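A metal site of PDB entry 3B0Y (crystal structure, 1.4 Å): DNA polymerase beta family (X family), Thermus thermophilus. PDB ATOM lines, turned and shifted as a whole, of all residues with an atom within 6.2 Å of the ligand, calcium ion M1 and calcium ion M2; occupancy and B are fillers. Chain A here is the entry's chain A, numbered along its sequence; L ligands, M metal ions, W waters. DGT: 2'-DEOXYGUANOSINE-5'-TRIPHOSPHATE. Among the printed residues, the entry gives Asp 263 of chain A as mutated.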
ATOM      1  N   ARG A 157      17.032  -4.385  24.070  1.00  0.00           N
ATOM      2  CA  ARG A 157      15.738  -4.785  24.643  1.00  0.00           C
ATOM      3  C   ARG A 157      15.995  -5.644  25.876  1.00  0.00           C
ATOM      4  O   ARG A 157      17.026  -6.319  25.984  1.00  0.00           O
ATOM      5  CB  ARG A 157      14.911  -5.524  23.589  1.00  0.00           C
ATOM      6  CG  ARG A 157      14.789  -4.703  22.297  1.00  0.00           C
ATOM      7  CD  ARG A 157      13.887  -5.344  21.263  1.00  0.00           C
ATOM      8  NE  ARG A 157      12.477  -5.409  21.676  1.00  0.00           N
ATOM      9  CZ  ARG A 157      11.606  -4.412  21.586  1.00  0.00           C
ATOM     10  NH1 ARG A 157      11.958  -3.246  21.037  1.00  0.00           N
ATOM     11  NH2 ARG A 157      10.369  -4.598  21.989  1.00  0.00           N
ATOM     12  N   CYS A 186       1.902   1.731  29.324  1.00  0.00           N
ATOM     13  CA  CYS A 186       1.439   1.445  27.964  1.00  0.00           C
ATOM     14  C   CYS A 186       2.568   0.832  27.119  1.00  0.00           C
ATOM     15  O   CYS A 186       3.294  -0.012  27.628  1.00  0.00           O
ATOM     16  CB  CYS A 186       0.810   2.686  27.333  1.00  0.00           C
ATOM     17  SG  CYS A 186      -0.654   3.302  28.230  1.00  0.00           S
ATOM     18  N   GLY A 187       2.692   1.238  25.863  1.00  0.00           N
ATOM     19  CA  GLY A 187       3.668   0.676  24.941  1.00  0.00           C
ATOM     20  C   GLY A 187       3.603  -0.838  24.846  1.00  0.00           C
ATOM     21  O   GLY A 187       2.585  -1.504  25.124  1.00  0.00           O
ATOM     22  N   SER A 188       4.730  -1.413  24.433  1.00  0.00           N
ATOM     23  CA  SER A 188       4.787  -2.863  24.220  1.00  0.00           C
ATOM     24  C   SER A 188       4.648  -3.678  25.493  1.00  0.00           C
ATOM     25  O   SER A 188       4.170  -4.825  25.447  1.00  0.00           O
ATOM     26  CB  SER A 188       6.072  -3.232  23.474  1.00  0.00           C
ATOM     27  OG  SER A 188       7.175  -2.864  24.297  1.00  0.00           O
ATOM     28  N   ALA A 189       4.960  -3.076  26.634  1.00  0.00           N
ATOM     29  CA  ALA A 189       4.755  -3.774  27.904  1.00  0.00           C
ATOM     30  C   ALA A 189       3.273  -4.096  28.112  1.00  0.00           C
ATOM     31  O   ALA A 189       2.911  -5.168  28.593  1.00  0.00           O
ATOM     32  CB  ALA A 189       5.251  -2.941  29.089  1.00  0.00           C
ATOM     33  N   ARG A 191       1.145  -4.662  25.913  1.00  0.00           N
ATOM     34  CA  ARG A 191       0.807  -5.712  24.939  1.00  0.00           C
ATOM     35  C   ARG A 191       1.449  -7.072  25.305  1.00  0.00           C
ATOM     36  O   ARG A 191       1.248  -8.032  24.583  1.00  0.00           O
ATOM     37  CB  ARG A 191       1.191  -5.299  23.521  1.00  0.00           C
ATOM     38  CG  ARG A 191       0.689  -3.908  23.123  1.00  0.00           C
ATOM     39  CD  ARG A 191       0.665  -3.706  21.595  1.00  0.00           C
ATOM     40  NE  ARG A 191       1.965  -4.023  20.998  1.00  0.00           N
ATOM     41  CZ  ARG A 191       2.989  -3.184  20.883  1.00  0.00           C
ATOM     42  NH1 ARG A 191       2.932  -1.924  21.349  1.00  0.00           N
ATOM     43  NH2 ARG A 191       4.127  -3.594  20.306  1.00  0.00           N
ATOM     44  N   LYS A 193       4.466  -8.036  25.115  1.00  0.00           N
ATOM     45  CA  LYS A 193       5.584  -8.431  24.247  1.00  0.00           C
ATOM     46  C   LYS A 193       6.713  -8.962  25.111  1.00  0.00           C
ATOM     47  O   LYS A 193       6.976  -8.412  26.191  1.00  0.00           O
ATOM     48  CB  LYS A 193       6.016  -7.223  23.431  1.00  0.00           C
ATOM     49  CG  LYS A 193       6.911  -7.603  22.252  1.00  0.00           C
ATOM     50  CD  LYS A 193       7.233  -6.362  21.451  1.00  0.00           C
ATOM     51  CE  LYS A 193       8.154  -6.673  20.279  1.00  0.00           C
ATOM     52  NZ  LYS A 193       7.396  -7.425  19.244  1.00  0.00           N
ATOM     53  N   THR A 195       9.966  -9.010  24.951  1.00  0.00           N
ATOM     54  CA  THR A 195      11.100  -8.092  25.187  1.00  0.00           C
ATOM     55  C   THR A 195      10.584  -6.715  24.895  1.00  0.00           C
ATOM     56  O   THR A 195       9.712  -6.538  24.027  1.00  0.00           O
ATOM     57  CB  THR A 195      12.364  -8.382  24.361  1.00  0.00           C
ATOM     58  OG1 THR A 195      12.119  -8.095  22.987  1.00  0.00           O
ATOM     59  CG2 THR A 195      12.785  -9.861  24.539  1.00  0.00           C
ATOM     60  N   VAL A 196      11.116  -5.744  25.621  1.00  0.00           N
ATOM     61  CA  VAL A 196      10.655  -4.356  25.510  1.00  0.00           C
ATOM     62  C   VAL A 196      11.813  -3.410  25.313  1.00  0.00           C
ATOM     63  O   VAL A 196      12.931  -3.652  25.820  1.00  0.00           O
ATOM     64  CB  VAL A 196       9.793  -3.916  26.709  1.00  0.00           C
ATOM     65  CG1 VAL A 196       8.529  -4.800  26.767  1.00  0.00           C
ATOM     66  CG2 VAL A 196      10.613  -3.969  28.011  1.00  0.00           C
ATOM     67  N   GLY A 197      11.558  -2.321  24.600  1.00  0.00           N
ATOM     68  CA  GLY A 197      12.506  -1.205  24.552  1.00  0.00           C
ATOM     69  C   GLY A 197      12.213  -0.293  25.728  1.00  0.00           C
ATOM     70  O   GLY A 197      12.110  -0.728  26.880  1.00  0.00           O
ATOM     71  N   ASP A 198      12.082   0.993  25.454  1.00  0.00           N
ATOM     72  CA  ASP A 198      11.761   1.910  26.535  1.00  0.00           C
ATOM     73  C   ASP A 198      10.357   1.632  27.113  1.00  0.00           C
ATOM     74  O   ASP A 198       9.529   0.957  26.470  1.00  0.00           O
ATOM     75  CB  ASP A 198      11.940   3.388  26.120  1.00  0.00           C
ATOM     76  CG  ASP A 198      10.951   3.850  25.077  1.00  0.00           C
ATOM     77  OD1 ASP A 198       9.914   3.212  24.823  1.00  0.00           O
ATOM     78  OD2 ASP A 198      11.188   4.918  24.480  1.00  0.00           O
ATOM     79  N   LEU A 199      10.118   2.143  28.318  1.00  0.00           N
ATOM     80  CA  LEU A 199       8.806   2.013  28.957  1.00  0.00           C
ATOM     81  C   LEU A 199       8.045   3.314  28.777  1.00  0.00           C
ATOM     82  O   LEU A 199       8.634   4.367  28.842  1.00  0.00           O
ATOM     83  CB  LEU A 199       8.975   1.712  30.444  1.00  0.00           C
ATOM     84  CG  LEU A 199       9.577   0.327  30.698  1.00  0.00           C
ATOM     85  CD1 LEU A 199      10.120   0.227  32.092  1.00  0.00           C
ATOM     86  CD2 LEU A 199       8.622  -0.790  30.384  1.00  0.00           C
ATOM     87  N   ASP A 200       6.739   3.219  28.540  1.00  0.00           N
ATOM     88  CA  ASP A 200       5.933   4.382  28.177  1.00  0.00           C
ATOM     89  C   ASP A 200       4.748   4.470  29.129  1.00  0.00           C
ATOM     90  O   ASP A 200       4.026   3.479  29.301  1.00  0.00           O
ATOM     91  CB  ASP A 200       5.387   4.170  26.756  1.00  0.00           C
ATOM     92  CG  ASP A 200       6.481   3.872  25.791  1.00  0.00           C
ATOM     93  OD1 ASP A 200       7.097   4.836  25.290  1.00  0.00           O
ATOM     94  OD2 ASP A 200       6.756   2.661  25.566  1.00  0.00           O
ATOM     95  N   ASP A 243       9.474   7.057  28.865  1.00  0.00           N
ATOM     96  CA  ASP A 243       8.743   8.134  28.242  1.00  0.00           C
ATOM     97  C   ASP A 243       7.434   8.342  29.005  1.00  0.00           C
ATOM     98  O   ASP A 243       6.758   7.380  29.379  1.00  0.00           O
ATOM     99  CB  ASP A 243       8.368   7.764  26.814  1.00  0.00           C
ATOM    100  CG  ASP A 243       9.533   7.810  25.843  1.00  0.00           C
ATOM    101  OD1 ASP A 243      10.561   8.429  26.120  1.00  0.00           O
ATOM    102  OD2 ASP A 243       9.359   7.230  24.756  1.00  0.00           O
ATOM    103  N   GLN A 257      -5.037   4.325  23.915  1.00  0.00           N
ATOM    104  CA  GLN A 257      -4.936   3.641  22.633  1.00  0.00           C
ATOM    105  C   GLN A 257      -3.643   4.095  21.921  1.00  0.00           C
ATOM    106  O   GLN A 257      -2.835   3.266  21.432  1.00  0.00           O
ATOM    107  CB  GLN A 257      -6.169   3.931  21.798  1.00  0.00           C
ATOM    108  CG  GLN A 257      -6.270   3.041  20.553  1.00  0.00           C
ATOM    109  CD  GLN A 257      -5.314   3.493  19.448  1.00  0.00           C
ATOM    110  OE1 GLN A 257      -5.238   4.672  19.095  1.00  0.00           O
ATOM    111  NE2 GLN A 257      -4.566   2.543  18.906  1.00  0.00           N
ATOM    112  N   TYR A 258      -3.425   5.408  21.871  1.00  0.00           N
ATOM    113  CA  TYR A 258      -2.277   5.956  21.154  1.00  0.00           C
ATOM    114  C   TYR A 258      -0.977   5.354  21.683  1.00  0.00           C
ATOM    115  O   TYR A 258      -0.105   4.937  20.905  1.00  0.00           O
ATOM    116  CB  TYR A 258      -2.274   7.483  21.333  1.00  0.00           C
ATOM    117  CG  TYR A 258      -1.059   8.155  20.758  1.00  0.00           C
ATOM    118  CD1 TYR A 258      -1.052   8.588  19.441  1.00  0.00           C
ATOM    119  CD2 TYR A 258       0.085   8.316  21.528  1.00  0.00           C
ATOM    120  CE1 TYR A 258       0.071   9.192  18.903  1.00  0.00           C
ATOM    121  CE2 TYR A 258       1.212   8.939  21.003  1.00  0.00           C
ATOM    122  CZ  TYR A 258       1.210   9.358  19.696  1.00  0.00           C
ATOM    123  OH  TYR A 258       2.332   9.944  19.153  1.00  0.00           O
ATOM    124  N   LEU A 259      -0.809   5.394  22.999  1.00  0.00           N
ATOM    125  CA  LEU A 259       0.468   5.042  23.580  1.00  0.00           C
ATOM    126  C   LEU A 259       0.689   3.526  23.690  1.00  0.00           C
ATOM    127  O   LEU A 259       1.801   3.094  23.970  1.00  0.00           O
ATOM    128  CB  LEU A 259       0.633   5.769  24.918  1.00  0.00           C
ATOM    129  CG  LEU A 259       2.085   5.848  25.397  1.00  0.00           C
ATOM    130  CD1 LEU A 259       3.006   6.420  24.379  1.00  0.00           C
ATOM    131  CD2 LEU A 259       2.216   6.545  26.739  1.00  0.00           C
ATOM    132  N   THR A 260      -0.382   2.749  23.520  1.00  0.00           N
ATOM    133  CA  THR A 260      -0.269   1.288  23.578  1.00  0.00           C
ATOM    134  C   THR A 260       0.085   0.701  22.220  1.00  0.00           C
ATOM    135  O   THR A 260       0.759  -0.321  22.143  1.00  0.00           O
ATOM    136  CB  THR A 260      -1.591   0.682  24.118  1.00  0.00           C
ATOM    137  OG1 THR A 260      -1.764   1.159  25.469  1.00  0.00           O
ATOM    138  CG2 THR A 260      -1.553  -0.856  24.136  1.00  0.00           C
ATOM    139  N   GLY A 261      -0.376   1.338  21.138  1.00  0.00           N
ATOM    140  CA  GLY A 261      -0.123   0.829  19.809  1.00  0.00           C
ATOM    141  C   GLY A 261      -0.602  -0.609  19.668  1.00  0.00           C
ATOM    142  O   GLY A 261      -1.617  -0.983  20.241  1.00  0.00           O
ATOM    143  N   SER A 262       0.110  -1.469  18.931  1.00  0.00           N
ATOM    144  CA  SER A 262       1.291  -1.135  18.143  1.00  0.00           C
ATOM    145  C   SER A 262       0.984  -0.053  17.117  1.00  0.00           C
ATOM    146  O   SER A 262      -0.192   0.259  16.822  1.00  0.00           O
ATOM    147  CB  SER A 262       1.736  -2.392  17.421  1.00  0.00           C
ATOM    148  OG  SER A 262       0.797  -2.722  16.399  1.00  0.00           O
ATOM    149  N   ASP A 263       2.036   0.501  16.526  1.00  0.00           N
ATOM    150  CA  ASP A 263       1.877   1.483  15.481  1.00  0.00           C
ATOM    151  C   ASP A 263       0.993   0.888  14.373  1.00  0.00           C
ATOM    152  O   ASP A 263       0.083   1.556  13.880  1.00  0.00           O
ATOM    153  CB  ASP A 263       3.256   1.870  14.943  1.00  0.00           C
ATOM    154  CG  ASP A 263       3.206   3.034  13.984  1.00  0.00           C
ATOM    155  OD1 ASP A 263       2.464   4.004  14.222  1.00  0.00           O
ATOM    156  OD2 ASP A 263       3.943   2.960  12.982  1.00  0.00           O
ATOM    157  N   SER A 266      -2.642   1.013  15.367  1.00  0.00           N
ATOM    158  CA  SER A 266      -3.175   2.374  15.372  1.00  0.00           C
ATOM    159  C   SER A 266      -3.385   2.866  13.935  1.00  0.00           C
ATOM    160  O   SER A 266      -4.351   3.570  13.666  1.00  0.00           O
ATOM    161  CB  SER A 266      -2.220   3.295  16.093  1.00  0.00           C
ATOM    162  OG  SER A 266      -2.128   2.922  17.445  1.00  0.00           O
HETATM  163  PG  DGT L   1       9.260  -0.962  22.008  1.00  0.00           P
HETATM  164  O1G DGT L   1       9.508   0.280  22.831  1.00  0.00           O
HETATM  165  O2G DGT L   1      10.166  -1.112  20.803  1.00  0.00           O
HETATM  166  O3G DGT L   1       9.239  -2.217  22.871  1.00  0.00           O
HETATM  167  O3B DGT L   1       7.744  -0.875  21.423  1.00  0.00           O
HETATM  168  PB  DGT L   1       6.603   0.205  21.699  1.00  0.00           P
HETATM  169  O1B DGT L   1       5.373  -0.255  21.008  1.00  0.00           O
HETATM  170  O2B DGT L   1       6.528   0.559  23.170  1.00  0.00           O
HETATM  171  O3A DGT L   1       7.102   1.491  20.879  1.00  0.00           O
HETATM  172  PA  DGT L   1       7.514   3.000  21.247  1.00  0.00           P
HETATM  173  O1A DGT L   1       8.009   3.089  22.659  1.00  0.00           O
HETATM  174  O2A DGT L   1       8.421   3.454  20.141  1.00  0.00           O
HETATM  175  O5' DGT L   1       6.173   3.799  21.072  1.00  0.00           O
HETATM  176  C5' DGT L   1       5.108   3.601  22.021  1.00  0.00           C
HETATM  177  C4' DGT L   1       3.773   3.648  21.295  1.00  0.00           C
HETATM  178  O4' DGT L   1       3.643   4.945  20.722  1.00  0.00           O
HETATM  179  C3' DGT L   1       3.624   2.693  20.111  1.00  0.00           C
HETATM  180  O3' DGT L   1       3.165   1.407  20.488  1.00  0.00           O
HETATM  181  C2' DGT L   1       2.569   3.380  19.244  1.00  0.00           C
HETATM  182  C1' DGT L   1       2.773   4.872  19.564  1.00  0.00           C
HETATM  183  N9  DGT L   1       3.425   5.566  18.437  1.00  0.00           N
HETATM  184  C8  DGT L   1       3.198   6.833  18.052  1.00  0.00           C
HETATM  185  N7  DGT L   1       3.978   7.148  16.991  1.00  0.00           N
HETATM  186  C5  DGT L   1       4.720   6.076  16.678  1.00  0.00           C
HETATM  187  C6  DGT L   1       5.744   5.728  15.659  1.00  0.00           C
HETATM  188  O6  DGT L   1       6.118   6.569  14.806  1.00  0.00           O
HETATM  189  N1  DGT L   1       6.263   4.483  15.674  1.00  0.00           N
HETATM  190  C2  DGT L   1       5.903   3.544  16.572  1.00  0.00           C
HETATM  191  N2  DGT L   1       6.460   2.295  16.534  1.00  0.00           N
HETATM  192  N3  DGT L   1       4.972   3.815  17.518  1.00  0.00           N
HETATM  193  C4  DGT L   1       4.364   5.028  17.617  1.00  0.00           C
HETATM  194 CA    CA M   1       8.850   5.186  23.730  1.00  0.00          CA
HETATM  195 CA    CA M   2       8.332   1.465  24.423  1.00  0.00          CA
HETATM  196  O   HOH W   1       7.546  -0.575  25.704  1.00  0.00           O
HETATM  197  O   HOH W   2      10.033   5.450  21.651  1.00  0.00           O
HETATM  198  O   HOH W   3       7.821   5.727  18.603  1.00  0.00           O
HETATM  199  O   HOH W   4       5.786   6.822  20.192  1.00  0.00           O
HETATM  200  O   HOH W   5      11.851   1.657  22.547  1.00  0.00           O
HETATM  201  O   HOH W   6       8.812  -2.594  18.789  1.00  0.00           O
HETATM  202  O   HOH W   7       7.249   6.553  22.546  1.00  0.00           O
HETATM  203  O   HOH W   8      -0.381   4.795  18.234  1.00  0.00           O
HETATM  204  O   HOH W   9       5.913  -2.032  18.883  1.00  0.00           O
HETATM  205  O   HOH W  10      11.467   0.486  19.054  1.00  0.00           O
HETATM  206  O   HOH W  11       4.699  -0.317  17.058  1.00  0.00           O
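OD2 of Asp 200 is bound to calcium ion M2, at 2.3 Å.
Calcium ion M2 is bound by O1G of the ligand (2.3 Å).
An oxygen (O2B) of the ligand is bound to calcium ion M2, 2.4 Å away.
The side-chain carboxylate (OD1) of Asp 198 binds calcium ion M2 (2.4 Å).
Calcium ion M2 is bound by O1A of the ligand, 2.4 Å away.
O of Asp 198 is bound to calcium ion M2 (2.4 Å).
Calcium ion M2 is bound by water W1, at 2.5 Å.
OD2 of Asp 243 binds calcium ion M1 (2.3 Å).
Calcium ion M1 is bound by the side-chain carboxylate (OD1) of Asp 200, 2.4 Å away.
Water W2 binds calcium ion M1.
Water W7 is bound to calcium ion M1 (2.4 Å).
Calcium ion M1 is bound by the side-chain carboxylate (OD2) of Asp 198, 2.5 Å away.
Calcium ion M1 is bound by OD1 of Asp 198 (2.5 Å).
O1A of the ligand is bound to calcium ion M1 (2.5 Å).
N of Ser 188 sits close to O2B of the ligand.
The side-chain hydroxyl of Ser 188 is in hydrogen-bond range of an oxygen (O3G) of the ligand, at 2.6 Å.
The guanidinium group of Arg 157 lies within salt-bridge range of an oxygen (O3G) of the ligand.
An oxygen (O3G) of the ligand is in hydrogen-bond range of the backbone NH of Gly 197, at 2.9 Å.
An oxygen (O1B) of the ligand lies within salt-bridge range of the guanidinium group (NH1) of Arg 191 (3.0 Å).
The backbone carbonyl oxygen (O) of Thr 260 lies within hydrogen-bond range of an oxygen (O3') of the ligand.
The backbone carbonyl oxygen (O) of Asp 200 sits at hydrogen-bond distance from the backbone NH (N) of Cys 186, 2.8 Å away.
The backbone NH of Asp 243 is in hydrogen-bond range of the backbone carbonyl oxygen of Leu 199 (2.8 Å).
O of Ser 188 lies within hydrogen-bond range of N of Lys 193 (3.2 Å).
The guanidinium group (NH2) of Arg 157 is in hydrogen-bond range of the backbone carbonyl oxygen (O) of Thr 195 (2.9 Å).
The backbone carbonyl oxygen of Thr 260 sits at hydrogen-bond distance from the guanidinium group of Arg 191 (2.8 Å).
The backbone NH (N) of Gly 187 is in hydrogen-bond range of the backbone carbonyl oxygen (O) of Leu 259, 2.8 Å away.
The side-chain hydroxyl (OG1) of Thr 260 sits close to the side-chain sulfur (SG) of Cys 186 (3.7 Å).
OG of Ser 266 sits at hydrogen-bond distance from O of Ser 262.
Water W9 bridges the guanidinium group of Arg 191 (2.8 Å) and an oxygen (O1B) of the ligand (2.8 Å).
Water W11 lies within hydrogen-bond range of N of Asp 263 and N2 of the ligand.
Water W8 lies within hydrogen-bond range of OG of Ser 266 and O of Tyr 258.
Of the 22 residues printed, 3 come within 4 Å of calcium ion M1.
Merely in contact with the ligand: Tyr 258 (3.2 Å), Gly 187 (3.4 Å), Leu 259 (3.4 Å), Gly 261 (3.4 Å), Asp 263 (3.5 Å), Val 196 (3.7 Å) and Ser 262 (3.9 Å).
Hydrophobic or aromatic side chains that line the ligand: Tyr 258 and Leu 259.
14 residues have an atom within 4 Å of the ligand: Arg 157, Gly 187, Ser 188, Arg 191, Val 196, Gly 197, Asp 198, Asp 200, Tyr 258, Leu 259, Thr 260, Gly 261, Ser 262 and Asp 263.
The nearest printed residue that does not touch the ligand is Thr 195 (4.5 Å).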
